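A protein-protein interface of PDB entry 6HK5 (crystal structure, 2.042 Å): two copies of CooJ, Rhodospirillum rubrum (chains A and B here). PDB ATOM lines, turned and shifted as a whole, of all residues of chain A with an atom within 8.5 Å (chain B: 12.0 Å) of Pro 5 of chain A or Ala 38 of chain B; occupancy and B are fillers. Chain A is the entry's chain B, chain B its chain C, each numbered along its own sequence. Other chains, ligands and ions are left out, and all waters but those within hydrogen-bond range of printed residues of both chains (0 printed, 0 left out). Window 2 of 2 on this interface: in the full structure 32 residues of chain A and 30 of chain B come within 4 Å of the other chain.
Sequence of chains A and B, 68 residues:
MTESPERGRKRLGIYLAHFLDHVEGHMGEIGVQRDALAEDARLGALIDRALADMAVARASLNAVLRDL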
ATOM      1  N   GLU A   3     -11.156  28.060  -4.165  1.00  0.00           N
ATOM      2  CA  GLU A   3      -9.811  28.611  -4.035  1.00  0.00           C
ATOM      3  C   GLU A   3      -8.773  27.529  -3.774  1.00  0.00           C
ATOM      4  O   GLU A   3      -9.057  26.515  -3.134  1.00  0.00           O
ATOM      5  CB  GLU A   3      -9.751  29.654  -2.912  1.00  0.00           C
ATOM      6  CG  GLU A   3      -9.826  29.091  -1.497  1.00  0.00           C
ATOM      7  CD  GLU A   3     -10.064  30.171  -0.445  1.00  0.00           C
ATOM      8  OE1 GLU A   3      -9.637  31.326  -0.661  1.00  0.00           O
ATOM      9  OE2 GLU A   3     -10.689  29.870   0.596  1.00  0.00           O
ATOM     10  N   SER A   4      -7.564  27.762  -4.287  1.00  0.00           N
ATOM     11  CA  SER A   4      -6.401  26.937  -4.006  1.00  0.00           C
ATOM     12  C   SER A   4      -6.200  26.840  -2.498  1.00  0.00           C
ATOM     13  O   SER A   4      -6.601  27.750  -1.757  1.00  0.00           O
ATOM     14  CB  SER A   4      -5.151  27.526  -4.662  1.00  0.00           C
ATOM     15  OG  SER A   4      -4.779  28.754  -4.041  1.00  0.00           O
ATOM     16  N   PRO A   5      -5.607  25.749  -2.008  1.00  0.00           N
ATOM     17  CA  PRO A   5      -5.270  25.682  -0.577  1.00  0.00           C
ATOM     18  C   PRO A   5      -4.415  26.839  -0.092  1.00  0.00           C
ATOM     19  O   PRO A   5      -4.579  27.264   1.057  1.00  0.00           O
ATOM     20  CB  PRO A   5      -4.541  24.337  -0.462  1.00  0.00           C
ATOM     21  CG  PRO A   5      -5.175  23.513  -1.526  1.00  0.00           C
ATOM     22  CD  PRO A   5      -5.418  24.451  -2.676  1.00  0.00           C
ATOM     23  N   GLU A   6      -3.520  27.376  -0.924  1.00  0.00           N
ATOM     24  CA  GLU A   6      -2.673  28.477  -0.480  1.00  0.00           C
ATOM     25  C   GLU A   6      -3.525  29.650   0.000  1.00  0.00           C
ATOM     26  O   GLU A   6      -3.392  30.102   1.142  1.00  0.00           O
ATOM     27  CB  GLU A   6      -1.727  28.901  -1.606  1.00  0.00           C
ATOM     28  CG  GLU A   6      -0.995  30.221  -1.369  1.00  0.00           C
ATOM     29  N   ARG A   7      -4.444  30.125  -0.849  1.00  0.00           N
ATOM     30  CA  ARG A   7      -5.285  31.268  -0.486  1.00  0.00           C
ATOM     31  C   ARG A   7      -6.215  30.932   0.678  1.00  0.00           C
ATOM     32  O   ARG A   7      -6.440  31.771   1.560  1.00  0.00           O
ATOM     33  CB  ARG A   7      -6.082  31.740  -1.709  1.00  0.00           C
ATOM     34  CG  ARG A   7      -6.993  32.956  -1.493  1.00  0.00           C
ATOM     35  CD  ARG A   7      -6.345  34.073  -0.677  1.00  0.00           C
ATOM     36  NE  ARG A   7      -7.174  35.282  -0.647  1.00  0.00           N
ATOM     37  CZ  ARG A   7      -7.289  36.099   0.403  1.00  0.00           C
ATOM     38  NH1 ARG A   7      -6.648  35.838   1.538  1.00  0.00           N
ATOM     39  NH2 ARG A   7      -8.065  37.173   0.326  1.00  0.00           N
ATOM     40  N   GLY A   8      -6.766  29.715   0.701  1.00  0.00           N
ATOM     41  CA  GLY A   8      -7.589  29.304   1.832  1.00  0.00           C
ATOM     42  C   GLY A   8      -6.877  29.440   3.167  1.00  0.00           C
ATOM     43  O   GLY A   8      -7.390  30.067   4.099  1.00  0.00           O
ATOM     44  N   ARG A   9      -5.680  28.856   3.283  1.00  0.00           N
ATOM     45  CA  ARG A   9      -4.965  28.928   4.554  1.00  0.00           C
ATOM     46  C   ARG A   9      -4.563  30.359   4.885  1.00  0.00           C
ATOM     47  O   ARG A   9      -4.536  30.741   6.058  1.00  0.00           O
ATOM     48  CB  ARG A   9      -3.742  28.014   4.524  1.00  0.00           C
ATOM     49  CG  ARG A   9      -4.092  26.570   4.290  1.00  0.00           C
ATOM     50  CD  ARG A   9      -2.869  25.750   3.972  1.00  0.00           C
ATOM     51  NE  ARG A   9      -3.232  24.344   3.867  1.00  0.00           N
ATOM     52  CZ  ARG A   9      -2.624  23.356   4.513  1.00  0.00           C
ATOM     53  NH1 ARG A   9      -1.583  23.609   5.302  1.00  0.00           N
ATOM     54  NH2 ARG A   9      -3.051  22.109   4.352  1.00  0.00           N
ATOM     55  N   LYS A  10      -4.286  31.158   3.858  1.00  0.00           N
ATOM     56  CA  LYS A  10      -3.977  32.577   4.039  1.00  0.00           C
ATOM     57  C   LYS A  10      -5.146  33.326   4.666  1.00  0.00           C
ATOM     58  O   LYS A  10      -4.993  34.008   5.694  1.00  0.00           O
ATOM     59  CB  LYS A  10      -3.616  33.171   2.676  1.00  0.00           C
ATOM     60  CG  LYS A  10      -3.437  34.683   2.614  1.00  0.00           C
ATOM     61  CD  LYS A  10      -1.987  35.069   2.296  1.00  0.00           C
ATOM     62  CE  LYS A  10      -1.875  36.531   1.902  1.00  0.00           C
ATOM     63  NZ  LYS A  10      -2.415  37.418   2.961  1.00  0.00           N
ATOM     64  N   ARG A  11      -6.334  33.216   4.068  1.00  0.00           N
ATOM     65  CA  ARG A  11      -7.500  33.919   4.585  1.00  0.00           C
ATOM     66  C   ARG A  11      -7.900  33.399   5.970  1.00  0.00           C
ATOM     67  O   ARG A  11      -8.292  34.178   6.847  1.00  0.00           O
ATOM     68  CB  ARG A  11      -8.644  33.800   3.569  1.00  0.00           C
ATOM     69  CG  ARG A  11     -10.044  33.994   4.110  1.00  0.00           C
ATOM     70  CD  ARG A  11     -11.020  33.063   3.413  1.00  0.00           C
ATOM     71  NE  ARG A  11     -10.506  31.697   3.370  1.00  0.00           N
ATOM     72  CZ  ARG A  11     -10.390  30.889   4.425  1.00  0.00           C
ATOM     73  NH1 ARG A  11      -9.900  29.666   4.262  1.00  0.00           N
ATOM     74  NH2 ARG A  11     -10.750  31.298   5.644  1.00  0.00           N
ATOM     75  N   LEU A  12      -7.783  32.089   6.201  1.00  0.00           N
ATOM     76  CA  LEU A  12      -8.105  31.567   7.526  1.00  0.00           C
ATOM     77  C   LEU A  12      -7.059  31.992   8.544  1.00  0.00           C
ATOM     78  O   LEU A  12      -7.398  32.377   9.670  1.00  0.00           O
ATOM     79  CB  LEU A  12      -8.238  30.052   7.477  1.00  0.00           C
ATOM     80  CG  LEU A  12      -8.426  29.397   8.836  1.00  0.00           C
ATOM     81  CD1 LEU A  12      -9.793  29.727   9.413  1.00  0.00           C
ATOM     82  CD2 LEU A  12      -8.249  27.899   8.699  1.00  0.00           C
ATOM     83  N   LEU A  68      -0.596  26.348   9.603  1.00  0.00           N
ATOM     84  CA  LEU A  68      -0.970  26.808   8.275  1.00  0.00           C
ATOM     85  C   LEU A  68       0.275  27.288   7.540  1.00  0.00           C
ATOM     86  O   LEU A  68       1.304  27.565   8.161  1.00  0.00           O
ATOM     87  CB  LEU A  68      -2.006  27.930   8.360  1.00  0.00           C
ATOM     88  CG  LEU A  68      -3.324  27.638   9.072  1.00  0.00           C
ATOM     89  CD1 LEU A  68      -4.091  28.927   9.308  1.00  0.00           C
ATOM     90  CD2 LEU A  68      -4.170  26.655   8.276  1.00  0.00           C
ATOM     91  N   ILE B  30     -14.845  27.696  11.143  1.00  0.00           N
ATOM     92  CA  ILE B  30     -13.959  26.591  10.803  1.00  0.00           C
ATOM     93  C   ILE B  30     -14.648  25.640   9.833  1.00  0.00           C
ATOM     94  O   ILE B  30     -14.078  25.244   8.808  1.00  0.00           O
ATOM     95  CB  ILE B  30     -13.501  25.879  12.089  1.00  0.00           C
ATOM     96  CG1 ILE B  30     -12.679  26.845  12.940  1.00  0.00           C
ATOM     97  CG2 ILE B  30     -12.738  24.579  11.789  1.00  0.00           C
ATOM     98  CD1 ILE B  30     -11.503  27.453  12.225  1.00  0.00           C
ATOM     99  N   GLY B  31     -15.896  25.280  10.134  1.00  0.00           N
ATOM    100  CA  GLY B  31     -16.639  24.394   9.249  1.00  0.00           C
ATOM    101  C   GLY B  31     -16.796  24.928   7.838  1.00  0.00           C
ATOM    102  O   GLY B  31     -16.809  24.157   6.874  1.00  0.00           O
ATOM    103  N   VAL B  32     -16.908  26.245   7.691  1.00  0.00           N
ATOM    104  CA  VAL B  32     -17.071  26.843   6.365  1.00  0.00           C
ATOM    105  C   VAL B  32     -15.743  26.898   5.620  1.00  0.00           C
ATOM    106  O   VAL B  32     -15.696  26.728   4.397  1.00  0.00           O
ATOM    107  CB  VAL B  32     -17.696  28.241   6.501  1.00  0.00           C
ATOM    108  CG1 VAL B  32     -17.519  29.051   5.220  1.00  0.00           C
ATOM    109  CG2 VAL B  32     -19.164  28.115   6.870  1.00  0.00           C
ATOM    110  N   GLN B  33     -14.645  27.139   6.324  1.00  0.00           N
ATOM    111  CA  GLN B  33     -13.386  27.367   5.632  1.00  0.00           C
ATOM    112  C   GLN B  33     -12.606  26.088   5.386  1.00  0.00           C
ATOM    113  O   GLN B  33     -11.657  26.102   4.593  1.00  0.00           O
ATOM    114  CB  GLN B  33     -12.518  28.347   6.428  1.00  0.00           C
ATOM    115  CG  GLN B  33     -13.245  29.612   6.886  1.00  0.00           C
ATOM    116  CD  GLN B  33     -13.577  30.579   5.746  1.00  0.00           C
ATOM    117  OE1 GLN B  33     -13.329  30.290   4.577  1.00  0.00           O
ATOM    118  NE2 GLN B  33     -14.127  31.744   6.094  1.00  0.00           N
ATOM    119  N   ARG B  34     -13.024  24.981   6.005  1.00  0.00           N
ATOM    120  CA  ARG B  34     -12.112  23.869   6.234  1.00  0.00           C
ATOM    121  C   ARG B  34     -11.715  23.181   4.934  1.00  0.00           C
ATOM    122  O   ARG B  34     -10.543  22.833   4.746  1.00  0.00           O
ATOM    123  CB  ARG B  34     -12.740  22.868   7.200  1.00  0.00           C
ATOM    124  CG  ARG B  34     -11.738  21.888   7.752  1.00  0.00           C
ATOM    125  CD  ARG B  34     -12.326  21.012   8.825  1.00  0.00           C
ATOM    126  NE  ARG B  34     -11.328  20.050   9.299  1.00  0.00           N
ATOM    127  CZ  ARG B  34     -11.467  19.302  10.389  1.00  0.00           C
ATOM    128  NH1 ARG B  34     -12.558  19.417  11.131  1.00  0.00           N
ATOM    129  NH2 ARG B  34     -10.510  18.451  10.748  1.00  0.00           N
ATOM    130  N   ASP B  35     -12.666  22.990   4.020  1.00  0.00           N
ATOM    131  CA  ASP B  35     -12.403  22.135   2.867  1.00  0.00           C
ATOM    132  C   ASP B  35     -11.324  22.720   1.967  1.00  0.00           C
ATOM    133  O   ASP B  35     -10.461  21.990   1.468  1.00  0.00           O
ATOM    134  CB  ASP B  35     -13.696  21.903   2.089  1.00  0.00           C
ATOM    135  CG  ASP B  35     -14.589  20.869   2.748  1.00  0.00           C
ATOM    136  OD1 ASP B  35     -15.760  20.760   2.327  1.00  0.00           O
ATOM    137  OD2 ASP B  35     -14.117  20.163   3.669  1.00  0.00           O
ATOM    138  N   ALA B  36     -11.335  24.023   1.774  1.00  0.00           N
ATOM    139  CA  ALA B  36     -10.339  24.669   0.928  1.00  0.00           C
ATOM    140  C   ALA B  36      -8.923  24.643   1.536  1.00  0.00           C
ATOM    141  O   ALA B  36      -7.990  25.209   0.959  1.00  0.00           O
ATOM    142  CB  ALA B  36     -10.768  26.109   0.637  1.00  0.00           C
ATOM    143  N   LEU B  37      -8.712  23.997   2.679  1.00  0.00           N
ATOM    144  CA  LEU B  37      -7.391  23.954   3.288  1.00  0.00           C
ATOM    145  C   LEU B  37      -6.530  22.816   2.757  1.00  0.00           C
ATOM    146  O   LEU B  37      -5.305  22.891   2.880  1.00  0.00           O
ATOM    147  CB  LEU B  37      -7.515  23.821   4.814  1.00  0.00           C
ATOM    148  CG  LEU B  37      -8.287  24.931   5.544  1.00  0.00           C
ATOM    149  CD1 LEU B  37      -8.325  24.643   7.026  1.00  0.00           C
ATOM    150  CD2 LEU B  37      -7.664  26.293   5.278  1.00  0.00           C
ATOM    151  N   ALA B  38      -7.145  21.778   2.176  1.00  0.00           N
ATOM    152  CA  ALA B  38      -6.454  20.546   1.758  1.00  0.00           C
ATOM    153  C   ALA B  38      -5.550  20.003   2.868  1.00  0.00           C
ATOM    154  O   ALA B  38      -4.357  19.746   2.674  1.00  0.00           O
ATOM    155  CB  ALA B  38      -5.669  20.763   0.464  1.00  0.00           C
ATOM    156  N   GLU B  39      -6.149  19.811   4.045  1.00  0.00           N
ATOM    157  CA  GLU B  39      -5.400  19.413   5.231  1.00  0.00           C
ATOM    158  C   GLU B  39      -4.828  18.004   5.090  1.00  0.00           C
ATOM    159  O   GLU B  39      -5.449  17.113   4.507  1.00  0.00           O
ATOM    160  CB  GLU B  39      -6.312  19.487   6.468  1.00  0.00           C
ATOM    161  CG  GLU B  39      -7.348  18.347   6.548  1.00  0.00           C
ATOM    162  CD  GLU B  39      -8.529  18.637   7.476  1.00  0.00           C
ATOM    163  OE1 GLU B  39      -9.153  19.715   7.348  1.00  0.00           O
ATOM    164  OE2 GLU B  39      -8.863  17.766   8.304  1.00  0.00           O
ATOM    165  N   ASP B  40      -3.637  17.806   5.634  1.00  0.00           N
ATOM    166  CA  ASP B  40      -3.133  16.465   5.868  1.00  0.00           C
ATOM    167  C   ASP B  40      -3.595  15.993   7.250  1.00  0.00           C
ATOM    168  O   ASP B  40      -4.325  16.697   7.955  1.00  0.00           O
ATOM    169  CB  ASP B  40      -1.613  16.430   5.727  1.00  0.00           C
ATOM    170  CG  ASP B  40      -0.889  17.308   6.752  1.00  0.00           C
ATOM    171  OD1 ASP B  40      -1.499  17.747   7.752  1.00  0.00           O
ATOM    172  OD2 ASP B  40       0.319  17.554   6.553  1.00  0.00           O
ATOM    173  N   ALA B  41      -3.150  14.799   7.660  1.00  0.00           N
ATOM    174  CA  ALA B  41      -3.632  14.234   8.918  1.00  0.00           C
ATOM    175  C   ALA B  41      -3.231  15.078  10.122  1.00  0.00           C
ATOM    176  O   ALA B  41      -3.910  15.039  11.155  1.00  0.00           O
ATOM    177  CB  ALA B  41      -3.114  12.806   9.101  1.00  0.00           C
ATOM    178  N   ARG B  42      -2.134  15.836  10.018  1.00  0.00           N
ATOM    179  CA  ARG B  42      -1.610  16.589  11.153  1.00  0.00           C
ATOM    180  C   ARG B  42      -2.375  17.890  11.367  1.00  0.00           C
ATOM    181  O   ARG B  42      -2.736  18.231  12.500  1.00  0.00           O
ATOM    182  CB  ARG B  42      -0.119  16.873  10.942  1.00  0.00           C
ATOM    183  CG  ARG B  42       0.452  17.989  11.794  1.00  0.00           C
ATOM    184  CD  ARG B  42       0.451  17.636  13.266  1.00  0.00           C
ATOM    185  N   LEU B  43      -2.620  18.638  10.291  1.00  0.00           N
ATOM    186  CA  LEU B  43      -3.457  19.819  10.410  1.00  0.00           C
ATOM    187  C   LEU B  43      -4.870  19.433  10.828  1.00  0.00           C
ATOM    188  O   LEU B  43      -5.488  20.113  11.663  1.00  0.00           O
ATOM    189  CB  LEU B  43      -3.458  20.595   9.093  1.00  0.00           C
ATOM    190  CG  LEU B  43      -4.320  21.851   9.131  1.00  0.00           C
ATOM    191  CD1 LEU B  43      -3.814  22.789  10.225  1.00  0.00           C
ATOM    192  CD2 LEU B  43      -4.284  22.535   7.800  1.00  0.00           C
ATOM    193  N   GLY B  44      -5.385  18.329  10.276  1.00  0.00           N
ATOM    194  CA  GLY B  44      -6.705  17.860  10.665  1.00  0.00           C
ATOM    195  C   GLY B  44      -6.788  17.537  12.142  1.00  0.00           C
ATOM    196  O   GLY B  44      -7.731  17.938  12.828  1.00  0.00           O
ATOM    197  N   ALA B  45      -5.793  16.807  12.655  1.00  0.00           N
ATOM    198  CA  ALA B  45      -5.745  16.511  14.079  1.00  0.00           C
ATOM    199  C   ALA B  45      -5.782  17.794  14.907  1.00  0.00           C
ATOM    200  O   ALA B  45      -6.520  17.883  15.892  1.00  0.00           O
ATOM    201  CB  ALA B  45      -4.490  15.691  14.399  1.00  0.00           C
ATOM    202  N   LEU B  46      -5.016  18.812  14.499  1.00  0.00           N
ATOM    203  CA  LEU B  46      -4.983  20.070  15.246  1.00  0.00           C
ATOM    204  C   LEU B  46      -6.315  20.811  15.162  1.00  0.00           C
ATOM    205  O   LEU B  46      -6.797  21.360  16.164  1.00  0.00           O
ATOM    206  CB  LEU B  46      -3.849  20.950  14.723  1.00  0.00           C
ATOM    207  CG  LEU B  46      -2.432  20.436  14.979  1.00  0.00           C
ATOM    208  CD1 LEU B  46      -1.426  21.306  14.258  1.00  0.00           C
ATOM    209  CD2 LEU B  46      -2.126  20.396  16.468  1.00  0.00           C
ATOM    210  N   ILE B  47      -6.910  20.858  13.969  1.00  0.00           N
ATOM    211  CA  ILE B  47      -8.220  21.483  13.824  1.00  0.00           C
ATOM    212  C   ILE B  47      -9.239  20.759  14.687  1.00  0.00           C
ATOM    213  O   ILE B  47      -9.948  21.377  15.482  1.00  0.00           O
ATOM    214  CB  ILE B  47      -8.644  21.515  12.344  1.00  0.00           C
ATOM    215  CG1 ILE B  47      -7.743  22.466  11.561  1.00  0.00           C
ATOM    216  CG2 ILE B  47     -10.108  21.919  12.216  1.00  0.00           C
ATOM    217  CD1 ILE B  47      -7.915  22.344  10.054  1.00  0.00           C
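The guanidinium group (NE) of Arg 9 of chain A is in hydrogen-bond range of the backbone carbonyl oxygen (O) of Leu 37 of chain B. NH2 of Arg 9 of chain A lies within hydrogen-bond range of O of Ala 38 of chain B. NH2 of Arg 11 of chain A lies close to OE1 of Gln 33 of chain B, 3.0 Å away.
OG of Ser 4 of chain A lies within hydrogen-bond range of N of Arg 7 of chain A. OD1 of Asp 40 of chain B lies within hydrogen-bond range of N of Leu 43 of chain B (2.9 Å). The backbone carbonyl oxygen (O) of Gly 8 of chain A lies within hydrogen-bond range of the guanidinium group (NH1) of Arg 11 of chain A, 2.5 Å away. The side-chain carboxylate of Glu 3 of chain A is in salt-bridge range of the guanidinium group of Arg 11 of chain A. NE of Arg 34 of chain B lies within salt-bridge range of OE1 of Glu 39 of chain B, 2.9 Å away.
Among the printed residues, pairs that only touch across the chains: Glu 3 of chain A with Ala 36 of chain B (3.8 Å), Ser 4 of chain A with Ala 36 of chain B (3.97 Å), Pro 5 of chain A with Ala 36 of chain B (3.2 Å), Pro 5 of chain A with Leu 37 of chain B (3.7 Å), Pro 5 of chain A with Ala 38 of chain B (3.4 Å), Gly 8 of chain A with Leu 37 of chain B (3.9 Å), Arg 9 of chain A with Glu 39 of chain B (3.7 Å), Arg 9 of chain A with Leu 43 of chain B (3.7 Å) and Leu 12 of chain A with Leu 37 of chain B (3.7 Å).
Ala 38 of chain B touches two residues of chain A. Of the printed residues of chain B, Ser 4 of chain A touches Ala 36. Of chain B, only Leu 37 (3.9 Å) comes within 4 Å of Gly 8 of chain A. Of chain B, only Leu 37 (2.7 Å), Ala 38 (3.2 Å), Glu 39 (3.7 Å) and Leu 43 (3.7 Å) come within 4 Å of Arg 9 of chain A. Printed residues of chain A within 4 Å of Leu 43 of chain B: Arg 9. Of the printed residues of chain B, Leu 12 of chain A touches Leu 37. Printed residues of chain A within 4 Å of Leu 37 of chain B: Pro 5 (3.7 Å), Gly 8 (3.9 Å), Arg 9 (2.7 Å) and Leu 12 (3.7 Å). Printed residues of chain A within 4 Å of Gln 33 of chain B: Arg 11 (2.9 Å).
Of the 18 printed residues of chain B, 6 touch a printed residue of chain A. Printed residues of chain B that touch a printed residue of chain A: Gln 33, Ala 36, Leu 37, Ala 38, Glu 39 and Leu 43. Printed residues of chain A that touch a printed residue of chain B: Glu 3, Ser 4, Pro 5, Gly 8, Arg 9, Arg 11 and Leu 12. Hydrophobic or aromatic side chains of chain A that line the printed part of chain B: Pro 5 and Leu 12. Among the printed residues, no Asp or Glu carboxylate lies within 4 Å of a Lys or Arg side-chain nitrogen of the other chain.
No position is printed for both chains.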
